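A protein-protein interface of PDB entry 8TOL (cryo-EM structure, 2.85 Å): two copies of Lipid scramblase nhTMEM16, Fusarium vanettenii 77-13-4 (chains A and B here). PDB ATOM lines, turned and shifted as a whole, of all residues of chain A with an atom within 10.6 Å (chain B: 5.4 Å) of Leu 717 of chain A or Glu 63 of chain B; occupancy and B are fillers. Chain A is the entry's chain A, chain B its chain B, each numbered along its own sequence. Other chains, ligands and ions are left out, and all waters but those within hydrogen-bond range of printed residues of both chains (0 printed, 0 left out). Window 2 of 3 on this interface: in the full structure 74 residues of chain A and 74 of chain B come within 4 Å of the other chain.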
ATOM      1  N   GLY A 709      10.664  25.096  30.751  1.00  0.00           N
ATOM      2  CA  GLY A 709       9.635  24.442  29.961  1.00  0.00           C
ATOM      3  C   GLY A 709       8.249  24.621  30.549  1.00  0.00           C
ATOM      4  O   GLY A 709       7.275  24.825  29.819  1.00  0.00           O
ATOM      5  N   ARG A 710       8.139  24.542  31.877  1.00  0.00           N
ATOM      6  CA  ARG A 710       6.856  24.781  32.530  1.00  0.00           C
ATOM      7  C   ARG A 710       6.386  26.212  32.298  1.00  0.00           C
ATOM      8  O   ARG A 710       5.237  26.451  31.896  1.00  0.00           O
ATOM      9  CB  ARG A 710       6.974  24.490  34.025  1.00  0.00           C
ATOM     10  CG  ARG A 710       5.758  23.820  34.628  1.00  0.00           C
ATOM     11  CD  ARG A 710       5.859  22.312  34.499  1.00  0.00           C
ATOM     12  NE  ARG A 710       6.860  21.756  35.400  1.00  0.00           N
ATOM     13  CZ  ARG A 710       6.892  20.491  35.796  1.00  0.00           C
ATOM     14  NH1 ARG A 710       5.990  19.616  35.385  1.00  0.00           N
ATOM     15  NH2 ARG A 710       7.853  20.095  36.627  1.00  0.00           N
ATOM     16  N   ARG A 711       7.268  27.182  32.555  1.00  0.00           N
ATOM     17  CA  ARG A 711       6.914  28.572  32.298  1.00  0.00           C
ATOM     18  C   ARG A 711       6.554  28.779  30.835  1.00  0.00           C
ATOM     19  O   ARG A 711       5.643  29.550  30.523  1.00  0.00           O
ATOM     20  CB  ARG A 711       8.063  29.494  32.701  1.00  0.00           C
ATOM     21  N   MET A 712       7.235  28.071  29.935  1.00  0.00           N
ATOM     22  CA  MET A 712       6.970  28.190  28.511  1.00  0.00           C
ATOM     23  C   MET A 712       5.584  27.666  28.162  1.00  0.00           C
ATOM     24  O   MET A 712       4.857  28.278  27.375  1.00  0.00           O
ATOM     25  CB  MET A 712       8.048  27.430  27.742  1.00  0.00           C
ATOM     26  CG  MET A 712       7.934  27.528  26.255  1.00  0.00           C
ATOM     27  SD  MET A 712       9.143  28.701  25.634  1.00  0.00           S
ATOM     28  CE  MET A 712       8.446  29.018  24.029  1.00  0.00           C
ATOM     29  N   ILE A 713       5.204  26.525  28.737  1.00  0.00           N
ATOM     30  CA  ILE A 713       3.893  25.946  28.451  1.00  0.00           C
ATOM     31  C   ILE A 713       2.783  26.854  28.963  1.00  0.00           C
ATOM     32  O   ILE A 713       1.799  27.119  28.257  1.00  0.00           O
ATOM     33  CB  ILE A 713       3.792  24.531  29.050  1.00  0.00           C
ATOM     34  CG1 ILE A 713       4.467  23.519  28.128  1.00  0.00           C
ATOM     35  CG2 ILE A 713       2.340  24.145  29.281  1.00  0.00           C
ATOM     36  CD1 ILE A 713       3.806  23.411  26.777  1.00  0.00           C
ATOM     37  N   GLU A 714       2.919  27.345  30.199  1.00  0.00           N
ATOM     38  CA  GLU A 714       1.902  28.252  30.731  1.00  0.00           C
ATOM     39  C   GLU A 714       1.857  29.573  29.968  1.00  0.00           C
ATOM     40  O   GLU A 714       0.777  30.140  29.773  1.00  0.00           O
ATOM     41  CB  GLU A 714       2.106  28.480  32.231  1.00  0.00           C
ATOM     42  CG  GLU A 714       1.866  27.245  33.118  1.00  0.00           C
ATOM     43  CD  GLU A 714       2.139  27.457  34.597  1.00  0.00           C
ATOM     44  OE1 GLU A 714       2.699  28.502  34.970  1.00  0.00           O
ATOM     45  OE2 GLU A 714       1.789  26.562  35.394  1.00  0.00           O
ATOM     46  N   GLN A 715       3.008  30.077  29.520  1.00  0.00           N
ATOM     47  CA  GLN A 715       3.002  31.280  28.693  1.00  0.00           C
ATOM     48  C   GLN A 715       2.318  31.030  27.356  1.00  0.00           C
ATOM     49  O   GLN A 715       1.565  31.881  26.867  1.00  0.00           O
ATOM     50  CB  GLN A 715       4.432  31.774  28.477  1.00  0.00           C
ATOM     51  CG  GLN A 715       4.535  32.984  27.568  1.00  0.00           C
ATOM     52  CD  GLN A 715       5.963  33.294  27.169  1.00  0.00           C
ATOM     53  OE1 GLN A 715       6.897  32.607  27.578  1.00  0.00           O
ATOM     54  NE2 GLN A 715       6.137  34.335  26.364  1.00  0.00           N
ATOM     55  N   GLN A 716       2.575  29.871  26.747  1.00  0.00           N
ATOM     56  CA  GLN A 716       1.984  29.558  25.451  1.00  0.00           C
ATOM     57  C   GLN A 716       0.473  29.415  25.551  1.00  0.00           C
ATOM     58  O   GLN A 716      -0.261  29.901  24.683  1.00  0.00           O
ATOM     59  CB  GLN A 716       2.607  28.280  24.890  1.00  0.00           C
ATOM     60  CG  GLN A 716       3.702  28.519  23.863  1.00  0.00           C
ATOM     61  CD  GLN A 716       3.811  27.392  22.857  1.00  0.00           C
ATOM     62  OE1 GLN A 716       3.043  26.431  22.898  1.00  0.00           O
ATOM     63  NE2 GLN A 716       4.772  27.502  21.947  1.00  0.00           N
ATOM     64  N   LEU A 717      -0.014  28.753  26.600  1.00  0.00           N
ATOM     65  CA  LEU A 717      -1.441  28.492  26.734  1.00  0.00           C
ATOM     66  C   LEU A 717      -2.118  29.404  27.751  1.00  0.00           C
ATOM     67  O   LEU A 717      -3.199  29.072  28.249  1.00  0.00           O
ATOM     68  CB  LEU A 717      -1.683  27.025  27.085  1.00  0.00           C
ATOM     69  CG  LEU A 717      -1.722  26.107  25.861  1.00  0.00           C
ATOM     70  CD1 LEU A 717      -2.537  24.860  26.137  1.00  0.00           C
ATOM     71  CD2 LEU A 717      -2.275  26.849  24.655  1.00  0.00           C
ATOM     72  N   ALA A 718      -1.508  30.541  28.069  1.00  0.00           N
ATOM     73  CA  ALA A 718      -2.149  31.558  28.889  1.00  0.00           C
ATOM     74  C   ALA A 718      -2.870  32.609  28.058  1.00  0.00           C
ATOM     75  O   ALA A 718      -3.439  33.546  28.627  1.00  0.00           O
ATOM     76  CB  ALA A 718      -1.116  32.236  29.795  1.00  0.00           C
ATOM     77  N   ALA A 719      -2.860  32.477  26.732  1.00  0.00           N
ATOM     78  CA  ALA A 719      -3.515  33.438  25.852  1.00  0.00           C
ATOM     79  C   ALA A 719      -4.911  32.968  25.452  1.00  0.00           C
ATOM     80  O   ALA A 719      -5.885  33.717  25.573  1.00  0.00           O
ATOM     81  CB  ALA A 719      -2.651  33.687  24.610  1.00  0.00           C
ATOM     82  N   GLY A 720      -5.020  31.732  24.976  1.00  0.00           N
ATOM     83  CA  GLY A 720      -6.299  31.184  24.567  1.00  0.00           C
ATOM     84  C   GLY A 720      -7.135  30.683  25.727  1.00  0.00           C
ATOM     85  O   GLY A 720      -7.562  31.463  26.579  1.00  0.00           O
ATOM     86  N   TYR B  27       6.761  17.759  19.309  1.00  0.00           N
ATOM     87  CA  TYR B  27       6.058  17.702  20.591  1.00  0.00           C
ATOM     88  C   TYR B  27       4.983  18.791  20.692  1.00  0.00           C
ATOM     89  O   TYR B  27       5.088  19.750  21.460  1.00  0.00           O
ATOM     90  CB  TYR B  27       7.030  17.789  21.772  1.00  0.00           C
ATOM     91  CG  TYR B  27       6.405  17.293  23.053  1.00  0.00           C
ATOM     92  CD1 TYR B  27       6.310  15.936  23.315  1.00  0.00           C
ATOM     93  CD2 TYR B  27       5.880  18.176  23.981  1.00  0.00           C
ATOM     94  CE1 TYR B  27       5.728  15.472  24.473  1.00  0.00           C
ATOM     95  CE2 TYR B  27       5.295  17.722  25.143  1.00  0.00           C
ATOM     96  CZ  TYR B  27       5.224  16.368  25.384  1.00  0.00           C
ATOM     97  OH  TYR B  27       4.642  15.906  26.539  1.00  0.00           O
ATOM     98  N   LYS B  28       3.947  18.626  19.870  1.00  0.00           N
ATOM     99  CA  LYS B  28       2.765  19.469  19.988  1.00  0.00           C
ATOM    100  C   LYS B  28       2.143  19.315  21.369  1.00  0.00           C
ATOM    101  O   LYS B  28       2.230  18.260  21.999  1.00  0.00           O
ATOM    102  CB  LYS B  28       1.741  19.106  18.910  1.00  0.00           C
ATOM    103  CG  LYS B  28       2.191  19.385  17.485  1.00  0.00           C
ATOM    104  CD  LYS B  28       1.139  20.172  16.720  1.00  0.00           C
ATOM    105  CE  LYS B  28       1.575  21.600  16.460  1.00  0.00           C
ATOM    106  NZ  LYS B  28       0.438  22.440  15.994  1.00  0.00           N
ATOM    107  N   VAL B  29       1.531  20.391  21.855  1.00  0.00           N
ATOM    108  CA  VAL B  29       0.837  20.354  23.141  1.00  0.00           C
ATOM    109  C   VAL B  29      -0.611  20.774  22.923  1.00  0.00           C
ATOM    110  O   VAL B  29      -0.902  21.975  22.820  1.00  0.00           O
ATOM    111  CB  VAL B  29       1.535  21.246  24.180  1.00  0.00           C
ATOM    112  CG1 VAL B  29       0.689  21.360  25.440  1.00  0.00           C
ATOM    113  CG2 VAL B  29       2.908  20.688  24.511  1.00  0.00           C
ATOM    114  N   PRO B  30      -1.543  19.830  22.826  1.00  0.00           N
ATOM    115  CA  PRO B  30      -2.947  20.196  22.619  1.00  0.00           C
ATOM    116  C   PRO B  30      -3.548  20.822  23.866  1.00  0.00           C
ATOM    117  O   PRO B  30      -3.038  20.682  24.981  1.00  0.00           O
ATOM    118  CB  PRO B  30      -3.624  18.860  22.288  1.00  0.00           C
ATOM    119  CG  PRO B  30      -2.504  17.878  22.060  1.00  0.00           C
ATOM    120  CD  PRO B  30      -1.353  18.373  22.866  1.00  0.00           C
ATOM    121  N   ALA B  31      -4.657  21.537  23.657  1.00  0.00           N
ATOM    122  CA  ALA B  31      -5.370  22.136  24.781  1.00  0.00           C
ATOM    123  C   ALA B  31      -5.885  21.065  25.734  1.00  0.00           C
ATOM    124  O   ALA B  31      -5.794  21.215  26.958  1.00  0.00           O
ATOM    125  CB  ALA B  31      -6.521  23.001  24.271  1.00  0.00           C
ATOM    126  N   ARG B  34      -3.680  18.521  29.091  1.00  0.00           N
ATOM    127  CA  ARG B  34      -2.538  19.350  29.460  1.00  0.00           C
ATOM    128  C   ARG B  34      -1.645  18.648  30.472  1.00  0.00           C
ATOM    129  O   ARG B  34      -0.414  18.699  30.368  1.00  0.00           O
ATOM    130  CB  ARG B  34      -3.015  20.690  30.016  1.00  0.00           C
ATOM    131  CG  ARG B  34      -3.310  21.723  28.954  1.00  0.00           C
ATOM    132  CD  ARG B  34      -2.075  22.564  28.675  1.00  0.00           C
ATOM    133  NE  ARG B  34      -1.343  22.923  29.885  1.00  0.00           N
ATOM    134  CZ  ARG B  34      -1.799  23.727  30.838  1.00  0.00           C
ATOM    135  NH1 ARG B  34      -2.981  24.311  30.746  1.00  0.00           N
ATOM    136  NH2 ARG B  34      -1.043  23.957  31.907  1.00  0.00           N
ATOM    137  N   GLU B  61       4.885  26.466  16.897  1.00  0.00           N
ATOM    138  CA  GLU B  61       4.173  27.295  15.930  1.00  0.00           C
ATOM    139  C   GLU B  61       3.013  28.066  16.574  1.00  0.00           C
ATOM    140  O   GLU B  61       3.042  29.300  16.609  1.00  0.00           O
ATOM    141  CB  GLU B  61       3.808  26.443  14.700  1.00  0.00           C
ATOM    142  CG  GLU B  61       2.973  25.157  14.865  1.00  0.00           C
ATOM    143  CD  GLU B  61       1.549  25.344  15.297  1.00  0.00           C
ATOM    144  OE1 GLU B  61       1.248  24.932  16.434  1.00  0.00           O
ATOM    145  OE2 GLU B  61       0.742  25.898  14.521  1.00  0.00           O
ATOM    146  N   ASN B  62       1.997  27.377  17.090  1.00  0.00           N
ATOM    147  CA  ASN B  62       1.141  27.996  18.101  1.00  0.00           C
ATOM    148  C   ASN B  62       0.776  27.067  19.249  1.00  0.00           C
ATOM    149  O   ASN B  62       0.438  27.565  20.328  1.00  0.00           O
ATOM    150  CB  ASN B  62      -0.143  28.579  17.483  1.00  0.00           C
ATOM    151  CG  ASN B  62      -1.101  27.524  16.950  1.00  0.00           C
ATOM    152  OD1 ASN B  62      -0.797  26.340  16.913  1.00  0.00           O
ATOM    153  ND2 ASN B  62      -2.278  27.970  16.525  1.00  0.00           N
ATOM    154  N   GLU B  63       0.840  25.746  19.072  1.00  0.00           N
ATOM    155  CA  GLU B  63       0.511  24.794  20.124  1.00  0.00           C
ATOM    156  C   GLU B  63       1.658  23.837  20.426  1.00  0.00           C
ATOM    157  O   GLU B  63       1.553  23.041  21.366  1.00  0.00           O
ATOM    158  CB  GLU B  63      -0.738  23.991  19.746  1.00  0.00           C
ATOM    159  CG  GLU B  63      -1.972  24.833  19.475  1.00  0.00           C
ATOM    160  CD  GLU B  63      -2.171  25.929  20.499  1.00  0.00           C
ATOM    161  OE1 GLU B  63      -2.211  25.612  21.704  1.00  0.00           O
ATOM    162  OE2 GLU B  63      -2.296  27.106  20.098  1.00  0.00           O
ATOM    163  N   SER B  64       2.741  23.890  19.660  1.00  0.00           N
ATOM    164  CA  SER B  64       3.833  22.936  19.770  1.00  0.00           C
ATOM    165  C   SER B  64       4.918  23.465  20.697  1.00  0.00           C
ATOM    166  O   SER B  64       4.916  24.628  21.109  1.00  0.00           O
ATOM    167  CB  SER B  64       4.420  22.625  18.389  1.00  0.00           C
ATOM    168  OG  SER B  64       4.557  23.803  17.616  1.00  0.00           O
ATOM    169  N   LEU B  65       5.858  22.577  21.027  1.00  0.00           N
ATOM    170  CA  LEU B  65       6.990  22.900  21.898  1.00  0.00           C
ATOM    171  C   LEU B  65       8.230  22.240  21.300  1.00  0.00           C
ATOM    172  O   LEU B  65       8.561  21.101  21.639  1.00  0.00           O
ATOM    173  CB  LEU B  65       6.734  22.433  23.323  1.00  0.00           C
ATOM    174  CG  LEU B  65       7.472  23.215  24.405  1.00  0.00           C
ATOM    175  CD1 LEU B  65       7.006  24.656  24.406  1.00  0.00           C
ATOM    176  CD2 LEU B  65       7.272  22.577  25.767  1.00  0.00           C
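The backbone NH of Leu 65 of chain B is in hydrogen-bond range of the backbone carbonyl oxygen of Tyr 27 of chain B (3.0 Å).
N of Val 29 of chain B is in hydrogen-bond range of O of Glu 63 of chain B (2.7 Å).
OE1 of Glu 61 of chain B sits close to OD1 of Asn 62 of chain B (2.5 Å).
The side-chain carboxylate (OE1) of Glu 61 of chain B lies within hydrogen-bond range of the backbone NH (N) of Glu 63 of chain B.
The backbone NH of Glu 61 of chain B sits at hydrogen-bond distance from the side-chain hydroxyl of Ser 64 of chain B.
No position is printed for both chains.
Of the 9 pairs that touch across the chains among the printed residues, none has its exchanged pair printed and touching as well.
Of the 11 printed residues of chain B, 6 touch a printed residue of chain A.
Hydrophobic or aromatic side chains of chain B within 4 Å of the printed part of chain A: Val 29 and Leu 65.
Of the 12 printed residues of chain A, 4 touch a printed residue of chain B.
Hydrophobic or aromatic side chains of chain A that line the printed part of chain B: Met 712, Ile 713 and Leu 717.
Among the printed residues, 9 pairs touch across the chains.
Of the printed residues of chain B, Met 712 of chain A touches Leu 65.
Of the printed residues of chain B, Ile 713 of chain A touches Val 29, Arg 34 and Leu 65.
Of the printed residues of chain B, Gln 716 of chain A touches Asn 62 (3.8 Å), Glu 63 (3.8 Å) and Ser 64 (3.0 Å).
Val 29 of chain B touches one residue of chain A.
No residue of chain A comes within 4 Å of Ala 31 of chain B.
Of the printed residues of chain A, Arg 34 of chain B touches Ile 713 (3.9 Å) and Leu 717 (3.5 Å).
Of the printed residues of chain A, Asn 62 of chain B touches Gln 716 (3.8 Å).
Printed residues of chain A within 4 Å of Glu 63 of chain B: Gln 716 and Leu 717.
Ser 64 of chain B touches one residue of chain A.
Printed residues of chain A within 4 Å of Leu 65 of chain B: Met 712 (3.5 Å) and Ile 713 (3.7 Å).
The nearest printed residue of chain A that does not touch Arg 34 of chain B is Glu 714 of chain A (4.6 Å).
The side-chain amide nitrogen (NE2) of Gln 716 of chain A lies within hydrogen-bond range of the backbone carbonyl oxygen (O) of Ser 64 of chain B, at 3.0 Å.
Among the printed residues, merely in contact across the chains: Met 712 of chain A with Leu 65 of chain B (3.5 Å), Ile 713 of chain A with Val 29 of chain B (3.7 Å), Ile 713 of chain A with Arg 34 of chain B (3.9 Å), Ile 713 of chain A with Leu 65 of chain B (3.7 Å), Gln 716 of chain A with Asn 62 of chain B (3.8 Å), Gln 716 of chain A with Glu 63 of chain B (3.8 Å), Leu 717 of chain A with Arg 34 of chain B (3.5 Å) and Leu 717 of chain A with Glu 63 of chain B (3.2 Å).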
